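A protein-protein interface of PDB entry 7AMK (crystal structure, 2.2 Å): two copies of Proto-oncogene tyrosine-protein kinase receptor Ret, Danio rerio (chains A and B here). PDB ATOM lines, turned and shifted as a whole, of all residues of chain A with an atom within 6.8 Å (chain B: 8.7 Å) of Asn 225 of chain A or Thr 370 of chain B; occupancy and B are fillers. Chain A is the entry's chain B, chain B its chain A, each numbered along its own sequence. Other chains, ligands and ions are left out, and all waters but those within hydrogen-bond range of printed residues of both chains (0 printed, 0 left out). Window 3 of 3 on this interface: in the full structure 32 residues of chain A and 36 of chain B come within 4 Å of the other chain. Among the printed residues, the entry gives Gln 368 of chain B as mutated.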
ATOM      1  N   ASN A 137      19.049  29.002  -2.699  1.00  0.00           N
ATOM      2  CA  ASN A 137      18.975  28.523  -1.325  1.00  0.00           C
ATOM      3  C   ASN A 137      19.995  29.279  -0.481  1.00  0.00           C
ATOM      4  O   ASN A 137      21.206  29.076  -0.651  1.00  0.00           O
ATOM      5  CB  ASN A 137      19.211  27.017  -1.266  1.00  0.00           C
ATOM      6  CG  ASN A 137      17.973  26.231  -1.660  1.00  0.00           C
ATOM      7  OD1 ASN A 137      16.838  26.731  -1.569  1.00  0.00           O
ATOM      8  ND2 ASN A 137      18.181  24.993  -2.093  1.00  0.00           N
ATOM      9  N   PRO A 138      19.577  30.178   0.385  1.00  0.00           N
ATOM     10  CA  PRO A 138      20.529  31.083   1.025  1.00  0.00           C
ATOM     11  C   PRO A 138      21.258  30.388   2.168  1.00  0.00           C
ATOM     12  O   PRO A 138      21.007  29.231   2.494  1.00  0.00           O
ATOM     13  CB  PRO A 138      19.638  32.219   1.511  1.00  0.00           C
ATOM     14  CG  PRO A 138      18.349  31.544   1.814  1.00  0.00           C
ATOM     15  CD  PRO A 138      18.189  30.508   0.733  1.00  0.00           C
ATOM     16  N   HIS A 139      22.194  31.113   2.757  1.00  0.00           N
ATOM     17  CA  HIS A 139      22.898  30.624   3.928  1.00  0.00           C
ATOM     18  C   HIS A 139      22.932  31.715   4.987  1.00  0.00           C
ATOM     19  O   HIS A 139      22.871  32.909   4.679  1.00  0.00           O
ATOM     20  CB  HIS A 139      24.325  30.188   3.590  1.00  0.00           C
ATOM     21  CG  HIS A 139      25.190  31.312   3.120  1.00  0.00           C
ATOM     22  ND1 HIS A 139      25.935  32.091   3.986  1.00  0.00           N
ATOM     23  CD2 HIS A 139      25.417  31.804   1.877  1.00  0.00           C
ATOM     24  CE1 HIS A 139      26.589  33.008   3.295  1.00  0.00           C
ATOM     25  NE2 HIS A 139      26.294  32.855   2.014  1.00  0.00           N
ATOM     26  N   ILE A 140      23.013  31.290   6.244  1.00  0.00           N
ATOM     27  CA  ILE A 140      23.203  32.202   7.362  1.00  0.00           C
ATOM     28  C   ILE A 140      24.234  31.568   8.281  1.00  0.00           C
ATOM     29  O   ILE A 140      24.424  30.350   8.273  1.00  0.00           O
ATOM     30  CB  ILE A 140      21.881  32.530   8.116  1.00  0.00           C
ATOM     31  CG1 ILE A 140      21.198  31.291   8.663  1.00  0.00           C
ATOM     32  CG2 ILE A 140      20.874  33.228   7.211  1.00  0.00           C
ATOM     33  CD1 ILE A 140      19.762  31.601   9.132  1.00  0.00           C
ATOM     34  N   THR A 141      24.932  32.402   9.051  1.00  0.00           N
ATOM     35  CA  THR A 141      26.008  31.924   9.907  1.00  0.00           C
ATOM     36  C   THR A 141      25.490  31.763  11.335  1.00  0.00           C
ATOM     37  O   THR A 141      24.726  32.597  11.833  1.00  0.00           O
ATOM     38  CB  THR A 141      27.220  32.866   9.849  1.00  0.00           C
ATOM     39  OG1 THR A 141      27.635  33.027   8.478  1.00  0.00           O
ATOM     40  CG2 THR A 141      28.402  32.290  10.627  1.00  0.00           C
ATOM     41  N   LYS A 198      21.059  22.313  14.189  1.00  0.00           N
ATOM     42  CA  LYS A 198      20.372  22.124  12.923  1.00  0.00           C
ATOM     43  C   LYS A 198      21.206  22.767  11.828  1.00  0.00           C
ATOM     44  O   LYS A 198      21.630  23.916  11.961  1.00  0.00           O
ATOM     45  CB  LYS A 198      18.958  22.710  12.955  1.00  0.00           C
ATOM     46  CG  LYS A 198      17.933  21.763  12.346  1.00  0.00           C
ATOM     47  CD  LYS A 198      16.614  22.458  12.088  1.00  0.00           C
ATOM     48  CE  LYS A 198      15.532  21.468  11.680  1.00  0.00           C
ATOM     49  NZ  LYS A 198      14.159  22.068  11.762  1.00  0.00           N
ATOM     50  N   GLU A 199      21.481  21.999  10.784  1.00  0.00           N
ATOM     51  CA  GLU A 199      22.363  22.420   9.712  1.00  0.00           C
ATOM     52  C   GLU A 199      21.611  22.948   8.501  1.00  0.00           C
ATOM     53  O   GLU A 199      22.199  23.680   7.696  1.00  0.00           O
ATOM     54  CB  GLU A 199      23.256  21.245   9.285  1.00  0.00           C
ATOM     55  CG  GLU A 199      24.548  21.661   8.583  1.00  0.00           C
ATOM     56  CD  GLU A 199      25.593  20.544   8.537  1.00  0.00           C
ATOM     57  OE1 GLU A 199      25.282  19.377   8.906  1.00  0.00           O
ATOM     58  OE2 GLU A 199      26.737  20.839   8.124  1.00  0.00           O
ATOM     59  N   VAL A 200      20.341  22.590   8.337  1.00  0.00           N
ATOM     60  CA  VAL A 200      19.559  23.112   7.213  1.00  0.00           C
ATOM     61  C   VAL A 200      18.093  23.163   7.619  1.00  0.00           C
ATOM     62  O   VAL A 200      17.613  22.342   8.402  1.00  0.00           O
ATOM     63  CB  VAL A 200      19.781  22.263   5.930  1.00  0.00           C
ATOM     64  CG1 VAL A 200      19.619  20.761   6.228  1.00  0.00           C
ATOM     65  CG2 VAL A 200      18.852  22.710   4.819  1.00  0.00           C
ATOM     66  N   TYR A 201      17.399  24.169   7.132  1.00  0.00           N
ATOM     67  CA  TYR A 201      15.982  24.323   7.359  1.00  0.00           C
ATOM     68  C   TYR A 201      15.260  24.197   6.028  1.00  0.00           C
ATOM     69  O   TYR A 201      15.760  24.655   4.999  1.00  0.00           O
ATOM     70  CB  TYR A 201      15.684  25.672   8.006  1.00  0.00           C
ATOM     71  CG  TYR A 201      16.130  25.773   9.428  1.00  0.00           C
ATOM     72  CD1 TYR A 201      17.429  26.139   9.746  1.00  0.00           C
ATOM     73  CD2 TYR A 201      15.248  25.495  10.475  1.00  0.00           C
ATOM     74  CE1 TYR A 201      17.844  26.238  11.096  1.00  0.00           C
ATOM     75  CE2 TYR A 201      15.654  25.582  11.793  1.00  0.00           C
ATOM     76  CZ  TYR A 201      16.950  25.951  12.101  1.00  0.00           C
ATOM     77  OH  TYR A 201      17.337  26.030  13.427  1.00  0.00           O
ATOM     78  N   HIS A 223      15.421  26.212   0.886  1.00  0.00           N
ATOM     79  CA  HIS A 223      16.295  25.610   1.888  1.00  0.00           C
ATOM     80  C   HIS A 223      17.305  26.638   2.354  1.00  0.00           C
ATOM     81  O   HIS A 223      17.885  27.357   1.539  1.00  0.00           O
ATOM     82  CB  HIS A 223      16.980  24.344   1.343  1.00  0.00           C
ATOM     83  CG  HIS A 223      16.013  23.385   0.708  1.00  0.00           C
ATOM     84  ND1 HIS A 223      15.301  22.451   1.431  1.00  0.00           N
ATOM     85  CD2 HIS A 223      15.582  23.270  -0.571  1.00  0.00           C
ATOM     86  CE1 HIS A 223      14.502  21.777   0.622  1.00  0.00           C
ATOM     87  NE2 HIS A 223      14.652  22.258  -0.600  1.00  0.00           N
ATOM     88  N   VAL A 224      17.456  26.758   3.665  1.00  0.00           N
ATOM     89  CA  VAL A 224      18.425  27.663   4.271  1.00  0.00           C
ATOM     90  C   VAL A 224      19.508  26.830   4.961  1.00  0.00           C
ATOM     91  O   VAL A 224      19.230  26.098   5.917  1.00  0.00           O
ATOM     92  CB  VAL A 224      17.765  28.623   5.272  1.00  0.00           C
ATOM     93  CG1 VAL A 224      18.848  29.527   5.862  1.00  0.00           C
ATOM     94  CG2 VAL A 224      16.611  29.466   4.605  1.00  0.00           C
ATOM     95  N   ASN A 225      20.730  26.956   4.475  1.00  0.00           N
ATOM     96  CA  ASN A 225      21.912  26.330   5.030  1.00  0.00           C
ATOM     97  C   ASN A 225      22.514  27.181   6.161  1.00  0.00           C
ATOM     98  O   ASN A 225      22.468  28.418   6.136  1.00  0.00           O
ATOM     99  CB  ASN A 225      22.937  26.116   3.917  1.00  0.00           C
ATOM    100  CG  ASN A 225      22.379  25.291   2.764  1.00  0.00           C
ATOM    101  OD1 ASN A 225      22.234  24.083   2.884  1.00  0.00           O
ATOM    102  ND2 ASN A 225      22.010  25.957   1.663  1.00  0.00           N
ATOM    103  N   ILE A 226      23.066  26.496   7.165  1.00  0.00           N
ATOM    104  CA  ILE A 226      23.709  27.140   8.316  1.00  0.00           C
ATOM    105  C   ILE A 226      25.210  26.898   8.211  1.00  0.00           C
ATOM    106  O   ILE A 226      25.664  25.744   8.220  1.00  0.00           O
ATOM    107  CB  ILE A 226      23.160  26.611   9.651  1.00  0.00           C
ATOM    108  CG1 ILE A 226      21.625  26.552   9.644  1.00  0.00           C
ATOM    109  CG2 ILE A 226      23.684  27.464  10.847  1.00  0.00           C
ATOM    110  CD1 ILE A 226      20.928  27.876   9.297  1.00  0.00           C
ATOM    111  N   TYR A 227      25.975  27.977   8.075  1.00  0.00           N
ATOM    112  CA  TYR A 227      27.431  27.878   8.019  1.00  0.00           C
ATOM    113  C   TYR A 227      27.996  27.627   9.419  1.00  0.00           C
ATOM    114  O   TYR A 227      27.587  28.260  10.397  1.00  0.00           O
ATOM    115  CB  TYR A 227      28.051  29.146   7.403  1.00  0.00           C
ATOM    116  CG  TYR A 227      27.992  29.193   5.887  1.00  0.00           C
ATOM    117  CD1 TYR A 227      27.300  28.231   5.170  1.00  0.00           C
ATOM    118  CD2 TYR A 227      28.632  30.196   5.172  1.00  0.00           C
ATOM    119  CE1 TYR A 227      27.225  28.270   3.785  1.00  0.00           C
ATOM    120  CE2 TYR A 227      28.572  30.244   3.771  1.00  0.00           C
ATOM    121  CZ  TYR A 227      27.871  29.277   3.090  1.00  0.00           C
ATOM    122  OH  TYR A 227      27.809  29.305   1.715  1.00  0.00           O
ATOM    123  N   PHE B 366      24.113  12.073  -0.229  1.00  0.00           N
ATOM    124  CA  PHE B 366      24.693  13.254   0.382  1.00  0.00           C
ATOM    125  C   PHE B 366      23.781  13.742   1.496  1.00  0.00           C
ATOM    126  O   PHE B 366      22.570  13.514   1.481  1.00  0.00           O
ATOM    127  CB  PHE B 366      24.882  14.372  -0.644  1.00  0.00           C
ATOM    128  CG  PHE B 366      25.921  14.087  -1.694  1.00  0.00           C
ATOM    129  CD1 PHE B 366      27.271  14.248  -1.417  1.00  0.00           C
ATOM    130  CD2 PHE B 366      25.546  13.710  -2.984  1.00  0.00           C
ATOM    131  CE1 PHE B 366      28.240  14.006  -2.397  1.00  0.00           C
ATOM    132  CE2 PHE B 366      26.509  13.466  -3.965  1.00  0.00           C
ATOM    133  CZ  PHE B 366      27.861  13.615  -3.663  1.00  0.00           C
ATOM    134  N   SER B 367      24.370  14.418   2.476  1.00  0.00           N
ATOM    135  CA  SER B 367      23.534  15.148   3.412  1.00  0.00           C
ATOM    136  C   SER B 367      22.673  16.141   2.642  1.00  0.00           C
ATOM    137  O   SER B 367      22.924  16.451   1.468  1.00  0.00           O
ATOM    138  CB  SER B 367      24.376  15.872   4.450  1.00  0.00           C
ATOM    139  OG  SER B 367      24.850  17.089   3.917  1.00  0.00           O
ATOM    140  N   GLN B 368      21.626  16.618   3.302  1.00  0.00           N
ATOM    141  CA  GLN B 368      20.775  17.614   2.673  1.00  0.00           C
ATOM    142  C   GLN B 368      21.382  19.014   2.731  1.00  0.00           C
ATOM    143  O   GLN B 368      20.716  19.978   2.338  1.00  0.00           O
ATOM    144  CB  GLN B 368      19.380  17.582   3.308  1.00  0.00           C
ATOM    145  CG  GLN B 368      19.368  17.362   4.809  1.00  0.00           C
ATOM    146  CD  GLN B 368      18.015  16.892   5.305  1.00  0.00           C
ATOM    147  OE1 GLN B 368      17.472  17.423   6.287  1.00  0.00           O
ATOM    148  NE2 GLN B 368      17.453  15.899   4.624  1.00  0.00           N
ATOM    149  N   VAL B 369      22.628  19.124   3.195  1.00  0.00           N
ATOM    150  CA  VAL B 369      23.370  20.384   3.208  1.00  0.00           C
ATOM    151  C   VAL B 369      24.183  20.477   1.920  1.00  0.00           C
ATOM    152  O   VAL B 369      25.193  19.785   1.766  1.00  0.00           O
ATOM    153  CB  VAL B 369      24.290  20.497   4.433  1.00  0.00           C
ATOM    154  CG1 VAL B 369      25.191  21.715   4.289  1.00  0.00           C
ATOM    155  CG2 VAL B 369      23.496  20.569   5.741  1.00  0.00           C
ATOM    156  N   THR B 370      23.778  21.375   1.022  1.00  0.00           N
ATOM    157  CA  THR B 370      24.499  21.585  -0.228  1.00  0.00           C
ATOM    158  C   THR B 370      25.821  22.324   0.003  1.00  0.00           C
ATOM    159  O   THR B 370      25.961  23.133   0.926  1.00  0.00           O
ATOM    160  CB  THR B 370      23.621  22.359  -1.209  1.00  0.00           C
ATOM    161  OG1 THR B 370      23.194  23.588  -0.606  1.00  0.00           O
ATOM    162  CG2 THR B 370      22.403  21.532  -1.596  1.00  0.00           C
ATOM    163  N   TYR B 371      26.794  22.050  -0.862  1.00  0.00           N
ATOM    164  CA  TYR B 371      28.123  22.615  -0.699  1.00  0.00           C
ATOM    165  C   TYR B 371      28.192  24.019  -1.292  1.00  0.00           C
ATOM    166  O   TYR B 371      27.625  24.296  -2.353  1.00  0.00           O
ATOM    167  CB  TYR B 371      29.176  21.738  -1.376  1.00  0.00           C
ATOM    168  CG  TYR B 371      29.319  20.332  -0.848  1.00  0.00           C
ATOM    169  CD1 TYR B 371      28.525  19.301  -1.334  1.00  0.00           C
ATOM    170  CD2 TYR B 371      30.279  20.023   0.113  1.00  0.00           C
ATOM    171  CE1 TYR B 371      28.675  18.010  -0.874  1.00  0.00           C
ATOM    172  CE2 TYR B 371      30.431  18.733   0.591  1.00  0.00           C
ATOM    173  CZ  TYR B 371      29.627  17.731   0.087  1.00  0.00           C
ATOM    174  OH  TYR B 371      29.770  16.441   0.529  1.00  0.00           O
ATOM    175  N   SER B 372      28.910  24.905  -0.611  1.00  0.00           N
ATOM    176  CA  SER B 372      29.269  26.198  -1.183  1.00  0.00           C
ATOM    177  C   SER B 372      30.699  26.502  -0.779  1.00  0.00           C
ATOM    178  O   SER B 372      31.009  26.573   0.412  1.00  0.00           O
ATOM    179  CB  SER B 372      28.321  27.312  -0.738  1.00  0.00           C
ATOM    180  OG  SER B 372      28.138  27.286   0.669  1.00  0.00           O
ATOM    181  N   PHE B 373      31.569  26.650  -1.768  1.00  0.00           N
ATOM    182  CA  PHE B 373      32.973  26.936  -1.541  1.00  0.00           C
ATOM    183  C   PHE B 373      33.271  28.339  -2.038  1.00  0.00           C
ATOM    184  O   PHE B 373      32.844  28.722  -3.137  1.00  0.00           O
ATOM    185  CB  PHE B 373      33.873  25.923  -2.252  1.00  0.00           C
ATOM    186  CG  PHE B 373      33.594  24.492  -1.894  1.00  0.00           C
ATOM    187  CD1 PHE B 373      33.875  24.012  -0.628  1.00  0.00           C
ATOM    188  CD2 PHE B 373      33.090  23.617  -2.844  1.00  0.00           C
ATOM    189  CE1 PHE B 373      33.631  22.684  -0.307  1.00  0.00           C
ATOM    190  CE2 PHE B 373      32.847  22.292  -2.531  1.00  0.00           C
ATOM    191  CZ  PHE B 373      33.111  21.826  -1.262  1.00  0.00           C
ATOM    192  N   VAL B 388      34.161  16.610  -1.529  1.00  0.00           N
ATOM    193  CA  VAL B 388      32.780  16.152  -1.562  1.00  0.00           C
ATOM    194  C   VAL B 388      32.767  14.698  -1.130  1.00  0.00           C
ATOM    195  O   VAL B 388      33.702  13.941  -1.410  1.00  0.00           O
ATOM    196  CB  VAL B 388      32.129  16.314  -2.954  1.00  0.00           C
ATOM    197  CG1 VAL B 388      32.050  17.787  -3.324  1.00  0.00           C
ATOM    198  CG2 VAL B 388      32.902  15.516  -4.010  1.00  0.00           C
ATOM    199  N   TYR B 454      27.016  23.993  -9.643  1.00  0.00           N
ATOM    200  CA  TYR B 454      27.176  22.651 -10.174  1.00  0.00           C
ATOM    201  C   TYR B 454      26.199  21.692  -9.514  1.00  0.00           C
ATOM    202  O   TYR B 454      25.630  21.960  -8.453  1.00  0.00           O
ATOM    203  CB  TYR B 454      28.592  22.112  -9.956  1.00  0.00           C
ATOM    204  CG  TYR B 454      29.706  22.833 -10.660  1.00  0.00           C
ATOM    205  CD1 TYR B 454      30.337  23.920 -10.065  1.00  0.00           C
ATOM    206  CD2 TYR B 454      30.168  22.407 -11.904  1.00  0.00           C
ATOM    207  CE1 TYR B 454      31.382  24.577 -10.697  1.00  0.00           C
ATOM    208  CE2 TYR B 454      31.215  23.058 -12.541  1.00  0.00           C
ATOM    209  CZ  TYR B 454      31.817  24.141 -11.929  1.00  0.00           C
ATOM    210  OH  TYR B 454      32.853  24.806 -12.541  1.00  0.00           O
ATOM    211  N   VAL B 456      26.759  17.841  -8.144  1.00  0.00           N
ATOM    212  CA  VAL B 456      27.700  16.762  -7.893  1.00  0.00           C
ATOM    213  C   VAL B 456      26.929  15.456  -7.905  1.00  0.00           C
ATOM    214  O   VAL B 456      25.853  15.349  -7.289  1.00  0.00           O
ATOM    215  CB  VAL B 456      28.436  16.942  -6.561  1.00  0.00           C
ATOM    216  CG1 VAL B 456      29.491  15.868  -6.446  1.00  0.00           C
ATOM    217  CG2 VAL B 456      29.030  18.346  -6.457  1.00  0.00           C
ATOM    218  N   LYS B 468      22.744  12.793  -5.724  1.00  0.00           N
ATOM    219  CA  LYS B 468      23.134  14.094  -6.231  1.00  0.00           C
ATOM    220  C   LYS B 468      23.055  15.106  -5.108  1.00  0.00           C
ATOM    221  O   LYS B 468      22.335  14.909  -4.125  1.00  0.00           O
ATOM    222  CB  LYS B 468      22.262  14.539  -7.413  1.00  0.00           C
ATOM    223  N   THR B 469      23.822  16.184  -5.259  1.00  0.00           N
ATOM    224  CA  THR B 469      23.659  17.360  -4.420  1.00  0.00           C
ATOM    225  C   THR B 469      24.096  18.581  -5.204  1.00  0.00           C
ATOM    226  O   THR B 469      24.736  18.466  -6.247  1.00  0.00           O
ATOM    227  CB  THR B 469      24.465  17.262  -3.116  1.00  0.00           C
ATOM    228  OG1 THR B 469      23.970  18.229  -2.187  1.00  0.00           O
ATOM    229  CG2 THR B 469      25.968  17.521  -3.367  1.00  0.00           C
ATOM    230  N   GLN B 470      23.746  19.753  -4.687  1.00  0.00           N
ATOM    231  CA  GLN B 470      24.070  21.005  -5.342  1.00  0.00           C
ATOM    232  C   GLN B 470      25.391  21.566  -4.822  1.00  0.00           C
ATOM    233  O   GLN B 470      25.798  21.319  -3.685  1.00  0.00           O
ATOM    234  CB  GLN B 470      22.945  22.019  -5.142  1.00  0.00           C
ATOM    235  CG  GLN B 470      21.719  21.734  -5.976  1.00  0.00           C
ATOM    236  N   LEU B 471      26.052  22.356  -5.657  1.00  0.00           N
ATOM    237  CA  LEU B 471      27.379  22.849  -5.293  1.00  0.00           C
ATOM    238  C   LEU B 471      27.604  24.200  -5.957  1.00  0.00           C
ATOM    239  O   LEU B 471      27.477  24.311  -7.184  1.00  0.00           O
ATOM    240  CB  LEU B 471      28.465  21.837  -5.705  1.00  0.00           C
ATOM    241  CG  LEU B 471      29.934  22.112  -5.372  1.00  0.00           C
ATOM    242  CD1 LEU B 471      30.720  20.800  -5.333  1.00  0.00           C
ATOM    243  CD2 LEU B 471      30.573  23.105  -6.352  1.00  0.00           C
ATOM    244  N   THR B 472      27.943  25.215  -5.154  1.00  0.00           N
ATOM    245  CA  THR B 472      28.286  26.537  -5.665  1.00  0.00           C
ATOM    246  C   THR B 472      29.727  26.887  -5.311  1.00  0.00           C
ATOM    247  O   THR B 472      30.193  26.607  -4.204  1.00  0.00           O
ATOM    248  CB  THR B 472      27.351  27.626  -5.121  1.00  0.00           C
ATOM    249  OG1 THR B 472      27.411  27.653  -3.690  1.00  0.00           O
ATOM    250  CG2 THR B 472      25.911  27.378  -5.569  1.00  0.00           C
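The backbone NH (N) of Val 369 of chain B sits close to the side-chain hydroxyl (OG) of Ser 367 of chain B (3.1 Å).
The backbone carbonyl oxygen (O) of Pro 138 of chain A lies within hydrogen-bond range of the backbone NH (N) of Asn 225 of chain A (3.0 Å).
The backbone NH (N) of Ile 140 of chain A sits at hydrogen-bond distance from the backbone carbonyl oxygen (O) of Asn 225 of chain A.
The backbone NH (N) of Tyr 227 of chain A sits at hydrogen-bond distance from the backbone carbonyl oxygen (O) of Ile 140 of chain A (2.8 Å).
O of Glu 199 of chain A is in hydrogen-bond range of N of Ile 226 of chain A (3.0 Å).
Glu 199 of chain A touches Val 369 of chain B.
Val 200 of chain A touches Gln 368 of chain B (CG1 to CG, 3.7 Å).
CG1 of Val 200 of chain A touches CG2 of Val 369 of chain B, 3.9 Å away.
CA of Val 369 of chain B touches OD1 of Asn 225 of chain A, at 3.9 Å.
Hydrophobic or aromatic side chains of chain B that line the printed part of chain A: Val 369.
Of the 14 printed residues of chain A, 4 touch a printed residue of chain B.
Printed residues of chain A that touch a printed residue of chain B: Glu 199, Val 200, Asn 225 and Tyr 227.
Hydrophobic or aromatic side chains of chain A within 4 Å of the printed part of chain B: Val 200 and Tyr 227.
No position is printed for both chains.
Of the 6 pairs that touch across the chains among the printed residues, none has its exchanged pair printed and touching as well.
Printed residues of chain B within 4 Å of Asn 225 of chain A: Val 369 and Thr 370.
Thr 370 of chain B touches just one residue of chain A: Asn 225.
Of the printed residues of chain B, Val 200 of chain A touches Gln 368 (3.7 Å) and Val 369 (3.9 Å).
Printed residues of chain A within 4 Å of Val 369 of chain B: Glu 199 (3.2 Å), Val 200 (3.9 Å) and Asn 225 (3.9 Å).
Printed residues of chain B within 4 Å of Glu 199 of chain A: Val 369 (3.2 Å).
Thr 141 of chain A touches none of the printed residues of chain B.
The nearest residue of chain B that does not touch Asn 225 of chain A is Gln 368 of chain B (4.4 Å).
The nearest printed residue of chain B that does not touch Tyr 227 of chain A is Thr 472 of chain B (5.7 Å).
The side-chain amide nitrogen (ND2) of Asn 225 of chain A sits at hydrogen-bond distance from the side-chain hydroxyl (OG1) of Thr 370 of chain B.
OG of Ser 372 of chain B sits close to OH of Tyr 227 of chain A.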
